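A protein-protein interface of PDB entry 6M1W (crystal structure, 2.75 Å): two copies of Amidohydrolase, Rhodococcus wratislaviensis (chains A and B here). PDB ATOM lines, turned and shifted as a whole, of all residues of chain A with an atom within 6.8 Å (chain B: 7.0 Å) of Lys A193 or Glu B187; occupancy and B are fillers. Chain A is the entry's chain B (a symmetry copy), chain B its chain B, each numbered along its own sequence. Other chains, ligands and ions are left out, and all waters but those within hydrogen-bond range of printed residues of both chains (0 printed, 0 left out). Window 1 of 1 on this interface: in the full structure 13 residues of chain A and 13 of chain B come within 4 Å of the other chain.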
ATOM      1  N   GLN A 124      -8.235  12.955  16.125  1.00  0.00           N
ATOM      2  CA  GLN A 124      -7.198  13.896  16.517  1.00  0.00           C
ATOM      3  C   GLN A 124      -7.648  15.341  16.320  1.00  0.00           C
ATOM      4  O   GLN A 124      -7.179  16.239  17.030  1.00  0.00           O
ATOM      5  CB  GLN A 124      -5.918  13.589  15.743  1.00  0.00           C
ATOM      6  CG  GLN A 124      -5.103  12.446  16.337  1.00  0.00           C
ATOM      7  CD  GLN A 124      -4.551  12.787  17.709  1.00  0.00           C
ATOM      8  OE1 GLN A 124      -3.515  13.459  17.843  1.00  0.00           O
ATOM      9  NE2 GLN A 124      -5.249  12.333  18.742  1.00  0.00           N
ATOM     10  N   PHE A 157       0.196  15.218  21.203  1.00  0.00           N
ATOM     11  CA  PHE A 157       1.543  14.732  20.939  1.00  0.00           C
ATOM     12  C   PHE A 157       1.591  13.717  19.805  1.00  0.00           C
ATOM     13  O   PHE A 157       2.693  13.351  19.391  1.00  0.00           O
ATOM     14  CB  PHE A 157       2.158  14.114  22.206  1.00  0.00           C
ATOM     15  CG  PHE A 157       3.110  15.027  22.940  1.00  0.00           C
ATOM     16  CD1 PHE A 157       2.635  16.062  23.729  1.00  0.00           C
ATOM     17  CD2 PHE A 157       4.477  14.848  22.846  1.00  0.00           C
ATOM     18  CE1 PHE A 157       3.505  16.909  24.403  1.00  0.00           C
ATOM     19  CE2 PHE A 157       5.353  15.695  23.511  1.00  0.00           C
ATOM     20  CZ  PHE A 157       4.861  16.726  24.293  1.00  0.00           C
ATOM     21  N   GLU A 158       0.449  13.259  19.278  1.00  0.00           N
ATOM     22  CA  GLU A 158       0.485  12.303  18.175  1.00  0.00           C
ATOM     23  C   GLU A 158       0.159  12.914  16.812  1.00  0.00           C
ATOM     24  O   GLU A 158       0.363  12.246  15.797  1.00  0.00           O
ATOM     25  CB  GLU A 158      -0.450  11.119  18.453  1.00  0.00           C
ATOM     26  CG  GLU A 158      -0.245  10.460  19.822  1.00  0.00           C
ATOM     27  CD  GLU A 158       0.963   9.512  19.909  1.00  0.00           C
ATOM     28  OE1 GLU A 158       2.000   9.753  19.249  1.00  0.00           O
ATOM     29  OE2 GLU A 158       0.870   8.514  20.667  1.00  0.00           O
ATOM     30  N   THR A 159      -0.332  14.150  16.747  1.00  0.00           N
ATOM     31  CA  THR A 159      -0.446  14.883  15.486  1.00  0.00           C
ATOM     32  C   THR A 159       0.384  16.152  15.634  1.00  0.00           C
ATOM     33  O   THR A 159      -0.140  17.219  15.999  1.00  0.00           O
ATOM     34  CB  THR A 159      -1.900  15.203  15.133  1.00  0.00           C
ATOM     35  OG1 THR A 159      -2.631  13.981  14.954  1.00  0.00           O
ATOM     36  CG2 THR A 159      -1.964  16.007  13.839  1.00  0.00           C
ATOM     37  N   PRO A 160       1.690  16.075  15.372  1.00  0.00           N
ATOM     38  CA  PRO A 160       2.581  17.204  15.711  1.00  0.00           C
ATOM     39  C   PRO A 160       2.183  18.520  15.073  1.00  0.00           C
ATOM     40  O   PRO A 160       2.438  19.579  15.662  1.00  0.00           O
ATOM     41  CB  PRO A 160       3.955  16.730  15.215  1.00  0.00           C
ATOM     42  CG  PRO A 160       3.855  15.210  15.187  1.00  0.00           C
ATOM     43  CD  PRO A 160       2.415  14.888  14.881  1.00  0.00           C
ATOM     44  N   LEU A 186       2.565   6.482  21.132  1.00  0.00           N
ATOM     45  CA  LEU A 186       2.570   5.393  20.164  1.00  0.00           C
ATOM     46  C   LEU A 186       3.985   4.983  19.783  1.00  0.00           C
ATOM     47  O   LEU A 186       4.229   3.801  19.502  1.00  0.00           O
ATOM     48  CB  LEU A 186       1.765   5.785  18.927  1.00  0.00           C
ATOM     49  CG  LEU A 186       1.365   4.634  18.003  1.00  0.00           C
ATOM     50  CD1 LEU A 186       0.378   3.667  18.649  1.00  0.00           C
ATOM     51  CD2 LEU A 186       0.779   5.227  16.761  1.00  0.00           C
ATOM     52  N   GLU A 187       4.919   5.924  19.784  1.00  0.00           N
ATOM     53  CA  GLU A 187       6.337   5.669  19.600  1.00  0.00           C
ATOM     54  C   GLU A 187       7.101   6.232  20.786  1.00  0.00           C
ATOM     55  O   GLU A 187       6.611   7.130  21.481  1.00  0.00           O
ATOM     56  CB  GLU A 187       6.872   6.320  18.317  1.00  0.00           C
ATOM     57  CG  GLU A 187       6.078   6.069  17.062  1.00  0.00           C
ATOM     58  CD  GLU A 187       6.752   6.676  15.844  1.00  0.00           C
ATOM     59  OE1 GLU A 187       8.001   6.646  15.772  1.00  0.00           O
ATOM     60  OE2 GLU A 187       6.038   7.194  14.961  1.00  0.00           O
ATOM     61  N   PRO A 188       8.302   5.742  21.044  1.00  0.00           N
ATOM     62  CA  PRO A 188       9.078   6.301  22.152  1.00  0.00           C
ATOM     63  C   PRO A 188       9.356   7.782  21.936  1.00  0.00           C
ATOM     64  O   PRO A 188       9.524   8.252  20.808  1.00  0.00           O
ATOM     65  CB  PRO A 188      10.358   5.463  22.145  1.00  0.00           C
ATOM     66  CG  PRO A 188       9.877   4.093  21.655  1.00  0.00           C
ATOM     67  CD  PRO A 188       8.845   4.449  20.584  1.00  0.00           C
ATOM     68  N   GLY A 190      11.697   9.738  22.140  1.00  0.00           N
ATOM     69  CA  GLY A 190      12.847  10.196  21.389  1.00  0.00           C
ATOM     70  C   GLY A 190      12.697  10.081  19.894  1.00  0.00           C
ATOM     71  O   GLY A 190      13.573  10.543  19.157  1.00  0.00           O
ATOM     72  N   SER A 191      11.608   9.471  19.433  1.00  0.00           N
ATOM     73  CA  SER A 191      11.407   9.306  18.004  1.00  0.00           C
ATOM     74  C   SER A 191      11.325  10.667  17.327  1.00  0.00           C
ATOM     75  O   SER A 191      11.110  11.696  17.966  1.00  0.00           O
ATOM     76  CB  SER A 191      10.145   8.496  17.726  1.00  0.00           C
ATOM     77  OG  SER A 191       9.583   8.874  16.481  1.00  0.00           O
ATOM     78  N   ARG A 192      11.508  10.675  16.017  1.00  0.00           N
ATOM     79  CA  ARG A 192      11.518  11.948  15.316  1.00  0.00           C
ATOM     80  C   ARG A 192      10.141  12.438  14.910  1.00  0.00           C
ATOM     81  O   ARG A 192      10.021  13.579  14.444  1.00  0.00           O
ATOM     82  CB  ARG A 192      12.401  11.872  14.097  1.00  0.00           C
ATOM     83  CG  ARG A 192      13.527  12.798  14.249  1.00  0.00           C
ATOM     84  CD  ARG A 192      14.044  13.222  12.948  1.00  0.00           C
ATOM     85  NE  ARG A 192      14.910  12.155  12.540  1.00  0.00           N
ATOM     86  CZ  ARG A 192      15.245  11.895  11.299  1.00  0.00           C
ATOM     87  NH1 ARG A 192      16.024  10.855  11.148  1.00  0.00           N
ATOM     88  NH2 ARG A 192      14.822  12.652  10.268  1.00  0.00           N
ATOM     89  N   LYS A 193       9.111  11.610  15.072  1.00  0.00           N
ATOM     90  CA  LYS A 193       7.745  12.091  14.929  1.00  0.00           C
ATOM     91  C   LYS A 193       7.497  13.301  15.819  1.00  0.00           C
ATOM     92  O   LYS A 193       6.779  14.232  15.424  1.00  0.00           O
ATOM     93  CB  LYS A 193       6.769  10.960  15.254  1.00  0.00           C
ATOM     94  CG  LYS A 193       5.437  11.404  15.803  1.00  0.00           C
ATOM     95  CD  LYS A 193       4.343  10.386  15.471  1.00  0.00           C
ATOM     96  CE  LYS A 193       3.114  10.609  16.325  1.00  0.00           C
ATOM     97  NZ  LYS A 193       1.894  10.048  15.692  1.00  0.00           N
ATOM     98  N   TYR A 194       8.119  13.326  17.006  1.00  0.00           N
ATOM     99  CA  TYR A 194       7.868  14.355  18.012  1.00  0.00           C
ATOM    100  C   TYR A 194       8.849  15.509  17.938  1.00  0.00           C
ATOM    101  O   TYR A 194       8.730  16.464  18.716  1.00  0.00           O
ATOM    102  CB  TYR A 194       7.911  13.748  19.418  1.00  0.00           C
ATOM    103  CG  TYR A 194       7.082  12.485  19.572  1.00  0.00           C
ATOM    104  CD1 TYR A 194       5.738  12.451  19.193  1.00  0.00           C
ATOM    105  CD2 TYR A 194       7.640  11.328  20.095  1.00  0.00           C
ATOM    106  CE1 TYR A 194       4.985  11.293  19.330  1.00  0.00           C
ATOM    107  CE2 TYR A 194       6.894  10.171  20.237  1.00  0.00           C
ATOM    108  CZ  TYR A 194       5.573  10.160  19.852  1.00  0.00           C
ATOM    109  OH  TYR A 194       4.849   9.008  19.990  1.00  0.00           O
ATOM    110  N   TRP A 195       9.815  15.443  17.048  1.00  0.00           N
ATOM    111  CA  TRP A 195      10.794  16.514  17.013  1.00  0.00           C
ATOM    112  C   TRP A 195      10.198  17.839  16.561  1.00  0.00           C
ATOM    113  O   TRP A 195      10.652  18.884  17.038  1.00  0.00           O
ATOM    114  CB  TRP A 195      11.968  16.124  16.130  1.00  0.00           C
ATOM    115  CG  TRP A 195      12.853  15.182  16.837  1.00  0.00           C
ATOM    116  CD1 TRP A 195      12.529  14.416  17.923  1.00  0.00           C
ATOM    117  CD2 TRP A 195      14.221  14.906  16.543  1.00  0.00           C
ATOM    118  NE1 TRP A 195      13.610  13.666  18.316  1.00  0.00           N
ATOM    119  CE2 TRP A 195      14.661  13.939  17.481  1.00  0.00           C
ATOM    120  CE3 TRP A 195      15.115  15.361  15.565  1.00  0.00           C
ATOM    121  CZ2 TRP A 195      15.955  13.432  17.477  1.00  0.00           C
ATOM    122  CZ3 TRP A 195      16.394  14.850  15.557  1.00  0.00           C
ATOM    123  CH2 TRP A 195      16.807  13.902  16.514  1.00  0.00           C
ATOM    124  N   PRO A 196       9.208  17.868  15.659  1.00  0.00           N
ATOM    125  CA  PRO A 196       8.564  19.159  15.375  1.00  0.00           C
ATOM    126  C   PRO A 196       7.991  19.811  16.616  1.00  0.00           C
ATOM    127  O   PRO A 196       7.995  21.044  16.711  1.00  0.00           O
ATOM    128  CB  PRO A 196       7.472  18.795  14.366  1.00  0.00           C
ATOM    129  CG  PRO A 196       7.992  17.584  13.679  1.00  0.00           C
ATOM    130  CD  PRO A 196       8.766  16.820  14.713  1.00  0.00           C
ATOM    131  N   ILE A 197       7.534  19.019  17.591  1.00  0.00           N
ATOM    132  CA  ILE A 197       6.974  19.580  18.822  1.00  0.00           C
ATOM    133  C   ILE A 197       8.070  20.154  19.713  1.00  0.00           C
ATOM    134  O   ILE A 197       7.854  21.159  20.407  1.00  0.00           O
ATOM    135  CB  ILE A 197       6.151  18.505  19.559  1.00  0.00           C
ATOM    136  CG1 ILE A 197       5.101  17.918  18.615  1.00  0.00           C
ATOM    137  CG2 ILE A 197       5.509  19.064  20.829  1.00  0.00           C
ATOM    138  CD1 ILE A 197       4.390  16.680  19.152  1.00  0.00           C
ATOM    139  N   GLU B 158       7.708   5.521   7.705  1.00  0.00           N
ATOM    140  CA  GLU B 158       7.508   5.874   9.108  1.00  0.00           C
ATOM    141  C   GLU B 158       8.330   7.079   9.569  1.00  0.00           C
ATOM    142  O   GLU B 158       8.082   7.584  10.663  1.00  0.00           O
ATOM    143  CB  GLU B 158       7.791   4.671  10.017  1.00  0.00           C
ATOM    144  CG  GLU B 158       7.056   3.389   9.614  1.00  0.00           C
ATOM    145  CD  GLU B 158       5.574   3.335  10.025  1.00  0.00           C
ATOM    146  OE1 GLU B 158       4.889   4.385  10.043  1.00  0.00           O
ATOM    147  OE2 GLU B 158       5.088   2.216  10.320  1.00  0.00           O
ATOM    148  N   THR B 159       9.289   7.559   8.779  1.00  0.00           N
ATOM    149  CA  THR B 159       9.953   8.837   9.040  1.00  0.00           C
ATOM    150  C   THR B 159       9.710   9.719   7.822  1.00  0.00           C
ATOM    151  O   THR B 159      10.541   9.775   6.898  1.00  0.00           O
ATOM    152  CB  THR B 159      11.447   8.665   9.319  1.00  0.00           C
ATOM    153  OG1 THR B 159      11.628   7.871  10.501  1.00  0.00           O
ATOM    154  CG2 THR B 159      12.102  10.025   9.537  1.00  0.00           C
ATOM    155  N   PRO B 160       8.573  10.416   7.775  1.00  0.00           N
ATOM    156  CA  PRO B 160       8.180  11.108   6.531  1.00  0.00           C
ATOM    157  C   PRO B 160       9.208  12.099   6.022  1.00  0.00           C
ATOM    158  O   PRO B 160       9.299  12.304   4.803  1.00  0.00           O
ATOM    159  CB  PRO B 160       6.867  11.806   6.915  1.00  0.00           C
ATOM    160  CG  PRO B 160       6.334  11.006   8.097  1.00  0.00           C
ATOM    161  CD  PRO B 160       7.541  10.477   8.827  1.00  0.00           C
ATOM    162  N   ASP B 161       9.988  12.722   6.914  1.00  0.00           N
ATOM    163  CA  ASP B 161      11.048  13.625   6.469  1.00  0.00           C
ATOM    164  C   ASP B 161      11.935  12.954   5.434  1.00  0.00           C
ATOM    165  O   ASP B 161      12.305  13.567   4.428  1.00  0.00           O
ATOM    166  CB  ASP B 161      11.904  14.077   7.652  1.00  0.00           C
ATOM    167  CG  ASP B 161      11.188  15.043   8.563  1.00  0.00           C
ATOM    168  OD1 ASP B 161      10.358  15.846   8.070  1.00  0.00           O
ATOM    169  OD2 ASP B 161      11.465  14.992   9.781  1.00  0.00           O
ATOM    170  N   LYS B 184       1.630  -3.066   5.932  1.00  0.00           N
ATOM    171  CA  LYS B 184       1.613  -2.933   7.381  1.00  0.00           C
ATOM    172  C   LYS B 184       2.418  -1.707   7.801  1.00  0.00           C
ATOM    173  O   LYS B 184       3.561  -1.518   7.365  1.00  0.00           O
ATOM    174  CB  LYS B 184       2.143  -4.209   8.044  1.00  0.00           C
ATOM    175  CG  LYS B 184       1.142  -5.361   7.925  1.00  0.00           C
ATOM    176  CD  LYS B 184       1.587  -6.606   8.656  1.00  0.00           C
ATOM    177  CE  LYS B 184       0.423  -7.563   8.865  1.00  0.00           C
ATOM    178  NZ  LYS B 184       0.015  -8.264   7.616  1.00  0.00           N
ATOM    179  N   THR B 185       1.801  -0.874   8.633  1.00  0.00           N
ATOM    180  CA  THR B 185       2.358   0.387   9.091  1.00  0.00           C
ATOM    181  C   THR B 185       2.003   0.557  10.559  1.00  0.00           C
ATOM    182  O   THR B 185       1.163  -0.168  11.102  1.00  0.00           O
ATOM    183  CB  THR B 185       1.820   1.566   8.284  1.00  0.00           C
ATOM    184  OG1 THR B 185       0.389   1.484   8.218  1.00  0.00           O
ATOM    185  CG2 THR B 185       2.396   1.559   6.885  1.00  0.00           C
ATOM    186  N   LEU B 186       2.649   1.524  11.210  1.00  0.00           N
ATOM    187  CA  LEU B 186       2.394   1.696  12.634  1.00  0.00           C
ATOM    188  C   LEU B 186       1.047   2.357  12.891  1.00  0.00           C
ATOM    189  O   LEU B 186       0.400   2.063  13.905  1.00  0.00           O
ATOM    190  CB  LEU B 186       3.524   2.496  13.279  1.00  0.00           C
ATOM    191  CG  LEU B 186       3.593   2.435  14.805  1.00  0.00           C
ATOM    192  CD1 LEU B 186       3.937   1.045  15.332  1.00  0.00           C
ATOM    193  CD2 LEU B 186       4.613   3.431  15.256  1.00  0.00           C
ATOM    194  N   GLU B 187       0.607   3.225  11.990  1.00  0.00           N
ATOM    195  CA  GLU B 187      -0.718   3.819  12.006  1.00  0.00           C
ATOM    196  C   GLU B 187      -1.407   3.530  10.682  1.00  0.00           C
ATOM    197  O   GLU B 187      -0.744   3.266   9.672  1.00  0.00           O
ATOM    198  CB  GLU B 187      -0.660   5.339  12.209  1.00  0.00           C
ATOM    199  CG  GLU B 187       0.199   5.826  13.346  1.00  0.00           C
ATOM    200  CD  GLU B 187       0.102   7.333  13.512  1.00  0.00           C
ATOM    201  OE1 GLU B 187      -1.004   7.888  13.324  1.00  0.00           O
ATOM    202  OE2 GLU B 187       1.131   7.968  13.822  1.00  0.00           O
ATOM    203  N   PRO B 188      -2.729   3.581  10.643  1.00  0.00           N
ATOM    204  CA  PRO B 188      -3.413   3.355   9.369  1.00  0.00           C
ATOM    205  C   PRO B 188      -3.003   4.392   8.333  1.00  0.00           C
ATOM    206  O   PRO B 188      -2.726   5.551   8.650  1.00  0.00           O
ATOM    207  CB  PRO B 188      -4.894   3.460   9.741  1.00  0.00           C
ATOM    208  CG  PRO B 188      -4.933   2.927  11.178  1.00  0.00           C
ATOM    209  CD  PRO B 188      -3.650   3.489  11.792  1.00  0.00           C
ATOM    210  N   LEU B 189      -2.967   3.948   7.073  1.00  0.00           N
ATOM    211  CA  LEU B 189      -2.368   4.747   6.008  1.00  0.00           C
ATOM    212  C   LEU B 189      -3.076   6.071   5.788  1.00  0.00           C
ATOM    213  O   LEU B 189      -2.492   6.974   5.182  1.00  0.00           O
ATOM    214  CB  LEU B 189      -2.342   3.955   4.703  1.00  0.00           C
ATOM    215  CG  LEU B 189      -1.054   3.138   4.642  1.00  0.00           C
ATOM    216  CD1 LEU B 189      -1.112   2.111   3.551  1.00  0.00           C
ATOM    217  CD2 LEU B 189       0.138   4.059   4.496  1.00  0.00           C
ATOM    218  N   GLY B 190      -4.314   6.209   6.253  1.00  0.00           N
ATOM    219  CA  GLY B 190      -4.990   7.484   6.141  1.00  0.00           C
ATOM    220  C   GLY B 190      -4.597   8.488   7.193  1.00  0.00           C
ATOM    221  O   GLY B 190      -5.032   9.641   7.128  1.00  0.00           O
ATOM    222  N   SER B 191      -3.788   8.072   8.165  1.00  0.00           N
ATOM    223  CA  SER B 191      -3.385   8.980   9.225  1.00  0.00           C
ATOM    224  C   SER B 191      -2.610  10.153   8.641  1.00  0.00           C
ATOM    225  O   SER B 191      -2.126  10.112   7.511  1.00  0.00           O
ATOM    226  CB  SER B 191      -2.542   8.252  10.268  1.00  0.00           C
ATOM    227  OG  SER B 191      -1.632   9.151  10.878  1.00  0.00           O
ATOM    228  N   ARG B 192      -2.500  11.219   9.418  1.00  0.00           N
ATOM    229  CA  ARG B 192      -1.838  12.403   8.896  1.00  0.00           C
ATOM    230  C   ARG B 192      -0.331  12.391   9.064  1.00  0.00           C
ATOM    231  O   ARG B 192       0.342  13.277   8.522  1.00  0.00           O
ATOM    232  CB  ARG B 192      -2.403  13.647   9.535  1.00  0.00           C
ATOM    233  CG  ARG B 192      -3.050  14.472   8.511  1.00  0.00           C
ATOM    234  CD  ARG B 192      -3.066  15.883   8.900  1.00  0.00           C
ATOM    235  NE  ARG B 192      -4.192  16.000   9.780  1.00  0.00           N
ATOM    236  CZ  ARG B 192      -4.341  16.939  10.683  1.00  0.00           C
ATOM    237  NH1 ARG B 192      -5.431  16.841  11.400  1.00  0.00           N
ATOM    238  NH2 ARG B 192      -3.441  17.928  10.846  1.00  0.00           N
ATOM    239  N   LYS B 193       0.207  11.419   9.798  1.00  0.00           N
ATOM    240  CA  LYS B 193       1.647  11.209   9.806  1.00  0.00           C
ATOM    241  C   LYS B 193       2.184  11.057   8.390  1.00  0.00           C
ATOM    242  O   LYS B 193       3.287  11.535   8.084  1.00  0.00           O
ATOM    243  CB  LYS B 193       1.978   9.981  10.655  1.00  0.00           C
ATOM    244  CG  LYS B 193       3.230   9.245  10.251  1.00  0.00           C
ATOM    245  CD  LYS B 193       3.849   8.521  11.449  1.00  0.00           C
ATOM    246  CE  LYS B 193       4.856   7.484  10.999  1.00  0.00           C
ATOM    247  NZ  LYS B 193       5.836   7.169  12.069  1.00  0.00           N
ATOM    248  N   TYR B 194       1.398  10.434   7.500  1.00  0.00           N
ATOM    249  CA  TYR B 194       1.839  10.101   6.149  1.00  0.00           C
ATOM    250  C   TYR B 194       1.461  11.154   5.124  1.00  0.00           C
ATOM    251  O   TYR B 194       1.802  11.008   3.944  1.00  0.00           O
ATOM    252  CB  TYR B 194       1.262   8.749   5.716  1.00  0.00           C
ATOM    253  CG  TYR B 194       1.444   7.643   6.740  1.00  0.00           C
ATOM    254  CD1 TYR B 194       2.700   7.355   7.279  1.00  0.00           C
ATOM    255  CD2 TYR B 194       0.362   6.887   7.169  1.00  0.00           C
ATOM    256  CE1 TYR B 194       2.861   6.347   8.220  1.00  0.00           C
ATOM    257  CE2 TYR B 194       0.517   5.878   8.105  1.00  0.00           C
ATOM    258  CZ  TYR B 194       1.764   5.616   8.625  1.00  0.00           C
ATOM    259  OH  TYR B 194       1.902   4.623   9.554  1.00  0.00           O
ATOM    260  N   GLY B 216       5.520  -4.001  10.648  1.00  0.00           N
ATOM    261  CA  GLY B 216       4.634  -2.869  10.830  1.00  0.00           C
ATOM    262  C   GLY B 216       4.599  -2.318  12.249  1.00  0.00           C
ATOM    263  O   GLY B 216       4.528  -1.096  12.442  1.00  0.00           O
ATOM    264  N   HIS B 218       2.456  -4.019  14.731  1.00  0.00           N
ATOM    265  CA  HIS B 218       1.345  -4.709  15.379  1.00  0.00           C
ATOM    266  C   HIS B 218       1.344  -6.190  14.996  1.00  0.00           C
ATOM    267  O   HIS B 218       2.153  -6.658  14.187  1.00  0.00           O
ATOM    268  CB  HIS B 218       0.008  -4.042  15.031  1.00  0.00           C
ATOM    269  CG  HIS B 218       0.000  -2.560  15.246  1.00  0.00           C
ATOM    270  ND1 HIS B 218      -0.073  -1.992  16.501  1.00  0.00           N
ATOM    271  CD2 HIS B 218       0.069  -1.530  14.367  1.00  0.00           C
ATOM    272  CE1 HIS B 218      -0.052  -0.675  16.385  1.00  0.00           C
ATOM    273  NE2 HIS B 218       0.033  -0.369  15.101  1.00  0.00           N
ATOM    274  N   GLN B 243      -6.369  -0.873   5.601  1.00  0.00           N
ATOM    275  CA  GLN B 243      -5.731   0.275   4.964  1.00  0.00           C
ATOM    276  C   GLN B 243      -6.689   0.976   4.026  1.00  0.00           C
ATOM    277  O   GLN B 243      -6.673   2.208   3.918  1.00  0.00           O
ATOM    278  CB  GLN B 243      -4.477  -0.133   4.189  1.00  0.00           C
ATOM    279  CG  GLN B 243      -3.349  -0.771   5.020  1.00  0.00           C
ATOM    280  CD  GLN B 243      -2.630   0.206   5.927  1.00  0.00           C
ATOM    281  OE1 GLN B 243      -3.080   1.338   6.139  1.00  0.00           O
ATOM    282  NE2 GLN B 243      -1.505  -0.231   6.477  1.00  0.00           N
ATOM    283  N   SER B 246      -9.206   3.098   6.043  1.00  0.00           N
ATOM    284  CA  SER B 246      -8.582   4.284   6.617  1.00  0.00           C
ATOM    285  C   SER B 246      -8.288   5.334   5.552  1.00  0.00           C
ATOM    286  O   SER B 246      -8.538   6.523   5.766  1.00  0.00           O
ATOM    287  CB  SER B 246      -7.306   3.899   7.350  1.00  0.00           C
ATOM    288  OG  SER B 246      -6.620   5.056   7.798  1.00  0.00           O
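Printed residues of chain B within 4 Å of Thr A159: Arg B192.
Printed residues of chain B within 4 Å of Leu A186: Glu B187 (3.5 Å).
Of the printed residues of chain B, Lys A193 touches Glu B187 (2.9 Å).
Of the printed residues of chain A, Leu B186 touches Glu A187 (3.5 Å).
Glu B187 touches two residues of chain A.
Printed residues of chain A within 4 Å of Lys B193: Glu A187.
The nearest residue of chain B that does not touch Lys A193 is Lys B193 (4.5 Å).
The nearest residue of chain A that does not touch Glu B187 is Glu A158 (4.8 Å).
The nearest printed residue of chain A that does not touch Lys B193 is Lys A193 (4.5 Å).
Thr A159 touches Arg B192, and with the chains exchanged Arg A192 touches Thr B159.
Leu A186 touches Glu B187, and with the chains exchanged Glu A187 touches Leu B186.
Glu A187 touches Lys B193, and with the chains exchanged Lys A193 touches Glu B187.
Among the printed residues, merely in contact across the chains: Thr A159 with Arg B192 (3.9 Å), Leu A186 with Glu B187 (3.5 Å), Glu A187 with Leu B186 (3.5 Å) and Arg A192 with Thr B159 (3.9 Å).
Of the 19 printed residues of chain B, 5 touch a printed residue of chain A.
Among the printed residues, Asp or Glu carboxylates within 4 Å of a Lys or Arg side-chain nitrogen of the other chain: Glu A187 with Lys B193 and Lys A193 with Glu B187.
NZ of Lys A193 lies within salt-bridge range of OE2 of Glu B187.
The side-chain carboxylate of Glu A187 lies within salt-bridge range of the side-chain amino group of Lys B193 (2.9 Å).
The side-chain carboxylate of Glu B158 lies within hydrogen-bond range of the backbone NH of Leu B186, 2.7 Å away.
N of Leu B186 sits at hydrogen-bond distance from O of Gly B216 (3.5 Å).
A ring nitrogen (NE2) of His B218 lies within hydrogen-bond range of the backbone carbonyl oxygen (O) of Leu B186 (2.7 Å).
The backbone carbonyl oxygen (O) of Glu B187 lies within hydrogen-bond range of the side-chain hydroxyl (OH) of Tyr B194 (3.0 Å).
The side-chain amide oxygen (OE1) of Gln A124 lies within hydrogen-bond range of the side-chain hydroxyl (OG1) of Thr A159 (3.1 Å).
The side-chain carboxylate of Glu A187 sits at hydrogen-bond distance from the side-chain hydroxyl of Ser A191, at 2.8 Å.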
